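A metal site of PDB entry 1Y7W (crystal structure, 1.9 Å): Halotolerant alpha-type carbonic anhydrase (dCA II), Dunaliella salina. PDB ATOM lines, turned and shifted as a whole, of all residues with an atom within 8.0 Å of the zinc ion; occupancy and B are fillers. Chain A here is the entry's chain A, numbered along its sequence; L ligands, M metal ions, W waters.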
ATOM      1  N   TYR A  25      -4.094  24.314   1.741  1.00  0.00           N
ATOM      2  CA  TYR A  25      -3.463  23.794   2.952  1.00  0.00           C
ATOM      3  C   TYR A  25      -1.969  23.698   2.903  1.00  0.00           C
ATOM      4  O   TYR A  25      -1.340  23.045   3.772  1.00  0.00           O
ATOM      5  CB  TYR A  25      -4.034  22.403   3.277  1.00  0.00           C
ATOM      6  CG  TYR A  25      -5.446  22.498   3.773  1.00  0.00           C
ATOM      7  CD1 TYR A  25      -6.536  22.432   2.880  1.00  0.00           C
ATOM      8  CD2 TYR A  25      -5.722  22.603   5.134  1.00  0.00           C
ATOM      9  CE1 TYR A  25      -7.869  22.448   3.360  1.00  0.00           C
ATOM     10  CE2 TYR A  25      -7.037  22.622   5.615  1.00  0.00           C
ATOM     11  CZ  TYR A  25      -8.094  22.533   4.734  1.00  0.00           C
ATOM     12  OH  TYR A  25      -9.383  22.458   5.262  1.00  0.00           O
ATOM     13  N   GLY A 100     -11.477  15.657   1.332  1.00  0.00           N
ATOM     14  CA  GLY A 100     -12.377  15.723   2.481  1.00  0.00           C
ATOM     15  C   GLY A 100     -13.538  14.742   2.485  1.00  0.00           C
ATOM     16  O   GLY A 100     -14.102  14.441   3.530  1.00  0.00           O
ATOM     17  N   GLN A 128     -23.973  17.272   7.641  1.00  0.00           N
ATOM     18  CA  GLN A 128     -22.987  16.575   6.748  1.00  0.00           C
ATOM     19  C   GLN A 128     -21.872  16.050   7.640  1.00  0.00           C
ATOM     20  O   GLN A 128     -21.831  16.392   8.839  1.00  0.00           O
ATOM     21  CB  GLN A 128     -22.375  17.567   5.762  1.00  0.00           C
ATOM     22  CG  GLN A 128     -21.822  18.860   6.430  1.00  0.00           C
ATOM     23  CD  GLN A 128     -20.329  18.972   6.338  1.00  0.00           C
ATOM     24  OE1 GLN A 128     -19.595  18.053   6.685  1.00  0.00           O
ATOM     25  NE2 GLN A 128     -19.859  20.108   5.884  1.00  0.00           N
ATOM     26  N   PHE A 129     -21.034  15.177   7.113  1.00  0.00           N
ATOM     27  CA  PHE A 129     -19.821  14.859   7.882  1.00  0.00           C
ATOM     28  C   PHE A 129     -18.691  14.850   6.869  1.00  0.00           C
ATOM     29  O   PHE A 129     -18.923  14.696   5.639  1.00  0.00           O
ATOM     30  CB  PHE A 129     -19.914  13.586   8.744  1.00  0.00           C
ATOM     31  CG  PHE A 129     -20.043  12.278   7.983  1.00  0.00           C
ATOM     32  CD1 PHE A 129     -18.959  11.686   7.377  1.00  0.00           C
ATOM     33  CD2 PHE A 129     -21.248  11.561   8.028  1.00  0.00           C
ATOM     34  CE1 PHE A 129     -19.029  10.386   6.819  1.00  0.00           C
ATOM     35  CE2 PHE A 129     -21.331  10.265   7.489  1.00  0.00           C
ATOM     36  CZ  PHE A 129     -20.225   9.682   6.891  1.00  0.00           C
ATOM     37  N   HIS A 130     -17.458  15.074   7.313  1.00  0.00           N
ATOM     38  CA  HIS A 130     -16.352  15.100   6.316  1.00  0.00           C
ATOM     39  C   HIS A 130     -15.071  14.671   7.030  1.00  0.00           C
ATOM     40  O   HIS A 130     -15.077  14.453   8.263  1.00  0.00           O
ATOM     41  CB  HIS A 130     -16.178  16.489   5.653  1.00  0.00           C
ATOM     42  CG  HIS A 130     -15.902  17.585   6.659  1.00  0.00           C
ATOM     43  ND1 HIS A 130     -16.901  18.359   7.230  1.00  0.00           N
ATOM     44  CD2 HIS A 130     -14.752  17.975   7.222  1.00  0.00           C
ATOM     45  CE1 HIS A 130     -16.359  19.177   8.131  1.00  0.00           C
ATOM     46  NE2 HIS A 130     -15.051  18.959   8.148  1.00  0.00           N
ATOM     47  N   PHE A 131     -13.978  14.612   6.290  1.00  0.00           N
ATOM     48  CA  PHE A 131     -12.742  14.103   6.896  1.00  0.00           C
ATOM     49  C   PHE A 131     -11.540  15.026   6.722  1.00  0.00           C
ATOM     50  O   PHE A 131     -11.443  15.782   5.751  1.00  0.00           O
ATOM     51  CB  PHE A 131     -12.342  12.764   6.249  1.00  0.00           C
ATOM     52  CG  PHE A 131     -13.343  11.642   6.412  1.00  0.00           C
ATOM     53  CD1 PHE A 131     -14.378  11.470   5.499  1.00  0.00           C
ATOM     54  CD2 PHE A 131     -13.243  10.776   7.506  1.00  0.00           C
ATOM     55  CE1 PHE A 131     -15.299  10.448   5.685  1.00  0.00           C
ATOM     56  CE2 PHE A 131     -14.146   9.748   7.716  1.00  0.00           C
ATOM     57  CZ  PHE A 131     -15.192   9.577   6.794  1.00  0.00           C
ATOM     58  N   HIS A 132     -10.592  14.897   7.655  1.00  0.00           N
ATOM     59  CA  HIS A 132      -9.312  15.636   7.541  1.00  0.00           C
ATOM     60  C   HIS A 132      -8.381  14.417   7.555  1.00  0.00           C
ATOM     61  O   HIS A 132      -8.320  13.665   8.535  1.00  0.00           O
ATOM     62  CB  HIS A 132      -9.135  16.588   8.720  1.00  0.00           C
ATOM     63  CG  HIS A 132     -10.100  17.739   8.669  1.00  0.00           C
ATOM     64  ND1 HIS A 132      -9.874  18.843   7.876  1.00  0.00           N
ATOM     65  CD2 HIS A 132     -11.356  17.879   9.169  1.00  0.00           C
ATOM     66  CE1 HIS A 132     -10.940  19.630   7.907  1.00  0.00           C
ATOM     67  NE2 HIS A 132     -11.852  19.074   8.679  1.00  0.00           N
ATOM     68  N   GLU A 137      -6.705  17.407  12.657  1.00  0.00           N
ATOM     69  CA  GLU A 137      -6.686  18.836  13.006  1.00  0.00           C
ATOM     70  C   GLU A 137      -6.443  18.962  14.518  1.00  0.00           C
ATOM     71  O   GLU A 137      -5.482  19.614  14.971  1.00  0.00           O
ATOM     72  CB  GLU A 137      -8.024  19.474  12.595  1.00  0.00           C
ATOM     73  CG  GLU A 137      -8.180  19.421  11.081  1.00  0.00           C
ATOM     74  CD  GLU A 137      -9.066  20.541  10.532  1.00  0.00           C
ATOM     75  OE1 GLU A 137     -10.216  20.684  11.003  1.00  0.00           O
ATOM     76  OE2 GLU A 137      -8.603  21.267   9.651  1.00  0.00           O
ATOM     77  N   HIS A 138      -7.293  18.346  15.329  1.00  0.00           N
ATOM     78  CA  HIS A 138      -6.989  18.380  16.775  1.00  0.00           C
ATOM     79  C   HIS A 138      -5.862  17.379  17.077  1.00  0.00           C
ATOM     80  O   HIS A 138      -5.638  16.455  16.283  1.00  0.00           O
ATOM     81  CB  HIS A 138      -8.169  17.954  17.646  1.00  0.00           C
ATOM     82  CG  HIS A 138      -9.285  18.927  17.626  1.00  0.00           C
ATOM     83  ND1 HIS A 138     -10.227  18.947  16.605  1.00  0.00           N
ATOM     84  CD2 HIS A 138      -9.575  19.976  18.445  1.00  0.00           C
ATOM     85  CE1 HIS A 138     -11.039  19.978  16.804  1.00  0.00           C
ATOM     86  NE2 HIS A 138     -10.668  20.624  17.891  1.00  0.00           N
ATOM     87  N   GLU A 148      -9.315  12.312  10.981  1.00  0.00           N
ATOM     88  CA  GLU A 148     -10.254  12.924  11.943  1.00  0.00           C
ATOM     89  C   GLU A 148     -11.544  13.190  11.167  1.00  0.00           C
ATOM     90  O   GLU A 148     -11.534  13.829  10.103  1.00  0.00           O
ATOM     91  CB  GLU A 148      -9.702  14.246  12.529  1.00  0.00           C
ATOM     92  CG  GLU A 148     -10.665  14.923  13.510  1.00  0.00           C
ATOM     93  CD  GLU A 148     -10.055  16.171  14.164  1.00  0.00           C
ATOM     94  OE1 GLU A 148      -8.799  16.255  14.239  1.00  0.00           O
ATOM     95  OE2 GLU A 148     -10.811  17.050  14.660  1.00  0.00           O
ATOM     96  N   LEU A 149     -12.621  12.628  11.702  1.00  0.00           N
ATOM     97  CA  LEU A 149     -13.957  12.770  11.150  1.00  0.00           C
ATOM     98  C   LEU A 149     -14.727  13.901  11.868  1.00  0.00           C
ATOM     99  O   LEU A 149     -14.710  13.979  13.086  1.00  0.00           O
ATOM    100  CB  LEU A 149     -14.700  11.444  11.358  1.00  0.00           C
ATOM    101  CG  LEU A 149     -16.252  11.486  11.359  1.00  0.00           C
ATOM    102  CD1 LEU A 149     -16.689  11.877   9.995  1.00  0.00           C
ATOM    103  CD2 LEU A 149     -16.827  10.080  11.700  1.00  0.00           C
ATOM    104  N   HIS A 150     -15.368  14.789  11.102  1.00  0.00           N
ATOM    105  CA  HIS A 150     -16.169  15.874  11.645  1.00  0.00           C
ATOM    106  C   HIS A 150     -17.647  15.704  11.217  1.00  0.00           C
ATOM    107  O   HIS A 150     -17.947  15.749  10.040  1.00  0.00           O
ATOM    108  CB  HIS A 150     -15.654  17.231  11.120  1.00  0.00           C
ATOM    109  CG  HIS A 150     -14.365  17.687  11.756  1.00  0.00           C
ATOM    110  ND1 HIS A 150     -13.569  18.697  11.221  1.00  0.00           N
ATOM    111  CD2 HIS A 150     -13.681  17.198  12.832  1.00  0.00           C
ATOM    112  CE1 HIS A 150     -12.453  18.788  11.928  1.00  0.00           C
ATOM    113  NE2 HIS A 150     -12.494  17.889  12.910  1.00  0.00           N
ATOM    114  N   ILE A 151     -18.522  15.448  12.180  1.00  0.00           N
ATOM    115  CA  ILE A 151     -19.973  15.371  11.965  1.00  0.00           C
ATOM    116  C   ILE A 151     -20.422  16.778  12.367  1.00  0.00           C
ATOM    117  O   ILE A 151     -20.303  17.182  13.550  1.00  0.00           O
ATOM    118  CB  ILE A 151     -20.654  14.354  12.871  1.00  0.00           C
ATOM    119  CG1 ILE A 151     -20.072  12.960  12.590  1.00  0.00           C
ATOM    120  CG2 ILE A 151     -22.184  14.342  12.580  1.00  0.00           C
ATOM    121  CD1 ILE A 151     -20.560  11.905  13.561  1.00  0.00           C
ATOM    122  N   VAL A 152     -20.915  17.520  11.390  1.00  0.00           N
ATOM    123  CA  VAL A 152     -21.306  18.920  11.569  1.00  0.00           C
ATOM    124  C   VAL A 152     -22.812  19.036  11.814  1.00  0.00           C
ATOM    125  O   VAL A 152     -23.565  18.482  11.022  1.00  0.00           O
ATOM    126  CB  VAL A 152     -21.001  19.696  10.309  1.00  0.00           C
ATOM    127  CG1 VAL A 152     -21.439  21.191  10.482  1.00  0.00           C
ATOM    128  CG2 VAL A 152     -19.441  19.613  10.014  1.00  0.00           C
ATOM    129  N   VAL A 168     -20.084  20.492  16.542  1.00  0.00           N
ATOM    130  CA  VAL A 168     -19.370  19.530  15.718  1.00  0.00           C
ATOM    131  C   VAL A 168     -18.787  18.416  16.597  1.00  0.00           C
ATOM    132  O   VAL A 168     -18.252  18.673  17.713  1.00  0.00           O
ATOM    133  CB  VAL A 168     -18.260  20.214  14.852  1.00  0.00           C
ATOM    134  CG1 VAL A 168     -17.421  19.110  14.050  1.00  0.00           C
ATOM    135  CG2 VAL A 168     -18.927  21.227  13.879  1.00  0.00           C
ATOM    136  N   ILE A 169     -18.890  17.192  16.099  1.00  0.00           N
ATOM    137  CA  ILE A 169     -18.382  16.044  16.792  1.00  0.00           C
ATOM    138  C   ILE A 169     -17.123  15.623  16.058  1.00  0.00           C
ATOM    139  O   ILE A 169     -17.142  15.488  14.846  1.00  0.00           O
ATOM    140  CB  ILE A 169     -19.416  14.918  16.790  1.00  0.00           C
ATOM    141  CG1 ILE A 169     -20.512  15.320  17.800  1.00  0.00           C
ATOM    142  CG2 ILE A 169     -18.799  13.598  17.173  1.00  0.00           C
ATOM    143  CD1 ILE A 169     -21.800  14.465  17.783  1.00  0.00           C
ATOM    144  N   SER A 230     -14.269  27.282  16.639  1.00  0.00           N
ATOM    145  CA  SER A 230     -14.596  27.826  15.351  1.00  0.00           C
ATOM    146  C   SER A 230     -14.622  26.836  14.221  1.00  0.00           C
ATOM    147  O   SER A 230     -14.266  25.677  14.407  1.00  0.00           O
ATOM    148  CB  SER A 230     -13.513  28.860  15.016  1.00  0.00           C
ATOM    149  OG  SER A 230     -12.311  28.245  14.499  1.00  0.00           O
ATOM    150  N   LEU A 231     -15.053  27.278  13.045  1.00  0.00           N
ATOM    151  CA  LEU A 231     -14.926  26.442  11.829  1.00  0.00           C
ATOM    152  C   LEU A 231     -13.391  26.339  11.656  1.00  0.00           C
ATOM    153  O   LEU A 231     -12.645  27.297  11.978  1.00  0.00           O
ATOM    154  CB  LEU A 231     -15.466  27.148  10.562  1.00  0.00           C
ATOM    155  CG  LEU A 231     -16.966  27.432  10.661  1.00  0.00           C
ATOM    156  CD1 LEU A 231     -17.463  28.237   9.471  1.00  0.00           C
ATOM    157  CD2 LEU A 231     -17.649  26.109  10.695  1.00  0.00           C
ATOM    158  N   THR A 232     -12.918  25.219  11.097  1.00  0.00           N
ATOM    159  CA  THR A 232     -11.462  25.084  10.872  1.00  0.00           C
ATOM    160  C   THR A 232     -11.092  25.387   9.395  1.00  0.00           C
ATOM    161  O   THR A 232     -10.005  25.099   8.957  1.00  0.00           O
ATOM    162  CB  THR A 232     -10.965  23.675  11.278  1.00  0.00           C
ATOM    163  OG1 THR A 232     -11.581  22.705  10.437  1.00  0.00           O
ATOM    164  CG2 THR A 232     -11.289  23.376  12.764  1.00  0.00           C
ATOM    165  N   THR A 233     -12.037  25.980   8.641  1.00  0.00           N
ATOM    166  CA  THR A 233     -11.806  26.407   7.286  1.00  0.00           C
ATOM    167  C   THR A 233     -12.278  27.846   7.249  1.00  0.00           C
ATOM    168  O   THR A 233     -13.146  28.234   8.074  1.00  0.00           O
ATOM    169  CB  THR A 233     -12.673  25.635   6.239  1.00  0.00           C
ATOM    170  OG1 THR A 233     -14.057  25.697   6.611  1.00  0.00           O
ATOM    171  CG2 THR A 233     -12.240  24.140   6.172  1.00  0.00           C
ATOM    172  N   TRP A 242     -17.504  22.461  20.168  1.00  0.00           N
ATOM    173  CA  TRP A 242     -16.751  21.291  19.759  1.00  0.00           C
ATOM    174  C   TRP A 242     -16.901  20.141  20.761  1.00  0.00           C
ATOM    175  O   TRP A 242     -16.981  20.364  21.980  1.00  0.00           O
ATOM    176  CB  TRP A 242     -15.235  21.644  19.593  1.00  0.00           C
ATOM    177  CG  TRP A 242     -14.939  22.236  18.232  1.00  0.00           C
ATOM    178  CD1 TRP A 242     -14.846  23.581  17.883  1.00  0.00           C
ATOM    179  CD2 TRP A 242     -14.750  21.499  17.053  1.00  0.00           C
ATOM    180  NE1 TRP A 242     -14.602  23.706  16.538  1.00  0.00           N
ATOM    181  CE2 TRP A 242     -14.536  22.433  15.999  1.00  0.00           C
ATOM    182  CE3 TRP A 242     -14.736  20.128  16.763  1.00  0.00           C
ATOM    183  CZ2 TRP A 242     -14.295  22.027  14.681  1.00  0.00           C
ATOM    184  CZ3 TRP A 242     -14.502  19.719  15.467  1.00  0.00           C
ATOM    185  CH2 TRP A 242     -14.281  20.678  14.432  1.00  0.00           C
ATOM    186  N   ASN A 274      -5.155  17.680   4.559  1.00  0.00           N
ATOM    187  CA  ASN A 274      -5.984  18.875   4.733  1.00  0.00           C
ATOM    188  C   ASN A 274      -6.354  19.294   6.141  1.00  0.00           C
ATOM    189  O   ASN A 274      -7.552  19.371   6.509  1.00  0.00           O
ATOM    190  CB  ASN A 274      -7.265  18.680   3.885  1.00  0.00           C
ATOM    191  CG  ASN A 274      -8.109  17.497   4.364  1.00  0.00           C
ATOM    192  OD1 ASN A 274      -7.561  16.500   4.858  1.00  0.00           O
ATOM    193  ND2 ASN A 274      -9.443  17.575   4.189  1.00  0.00           N
HETATM  194  C1  LIG L   1     -15.692  22.306  10.757  1.00  0.00           C
HETATM  195  O1  LIG L   1     -15.447  21.029  10.735  1.00  0.00           O
HETATM  196  O2  LIG L   1     -14.813  23.167  10.720  1.00  0.00           O
HETATM  197  C2  LIG L   1     -17.169  22.664  10.807  1.00  0.00           C
HETATM  198 ZN    ZN M   1     -13.687  19.657   9.425  1.00  0.00          ZN
HETATM  199  O   HOH W   1     -13.499  21.488   8.910  1.00  0.00           O
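Glu 137 touches the zinc ion (OE1 to ZN, 3.9 Å).
Thr 232 touches the zinc ion.
Of the 22 residues printed, 5 come within 4 Å of the zinc ion.
The zinc ion is bound by water W1 (1.9 Å).
The zinc ion is bound by a ring nitrogen (NE2) of His 130 (2.0 Å).
ND1 of His 150 binds the zinc ion (2.0 Å).
NE2 of His 132 binds the zinc ion (2.1 Å).
O1 of the ligand is bound to the zinc ion (2.6 Å).
The zinc ion has five donor atoms within binding distance.
A ring nitrogen (ND1) of His 132 lies close to the side-chain carboxylate (OE2) of Glu 137, 3.3 Å away.
The side-chain carboxylate (OE1) of Glu 148 sits at hydrogen-bond distance from the backbone NH (N) of Glu 137 (2.9 Å).
A ring nitrogen (ND1) of His 132 is in hydrogen-bond range of the backbone carbonyl oxygen of Asn 274, at 2.7 Å.
The backbone NH (N) of His 132 is in hydrogen-bond range of the backbone carbonyl oxygen (O) of Glu 148 (2.8 Å).
The side-chain carboxylate of Glu 137 is in hydrogen-bond range of the side-chain hydroxyl of Thr 232.
NE2 of His 150 lies within hydrogen-bond range of OE2 of Glu 148, 2.6 Å away.
The side-chain amide oxygen (OE1) of Gln 128 lies within hydrogen-bond range of a ring nitrogen (ND1) of His 130, at 2.8 Å.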
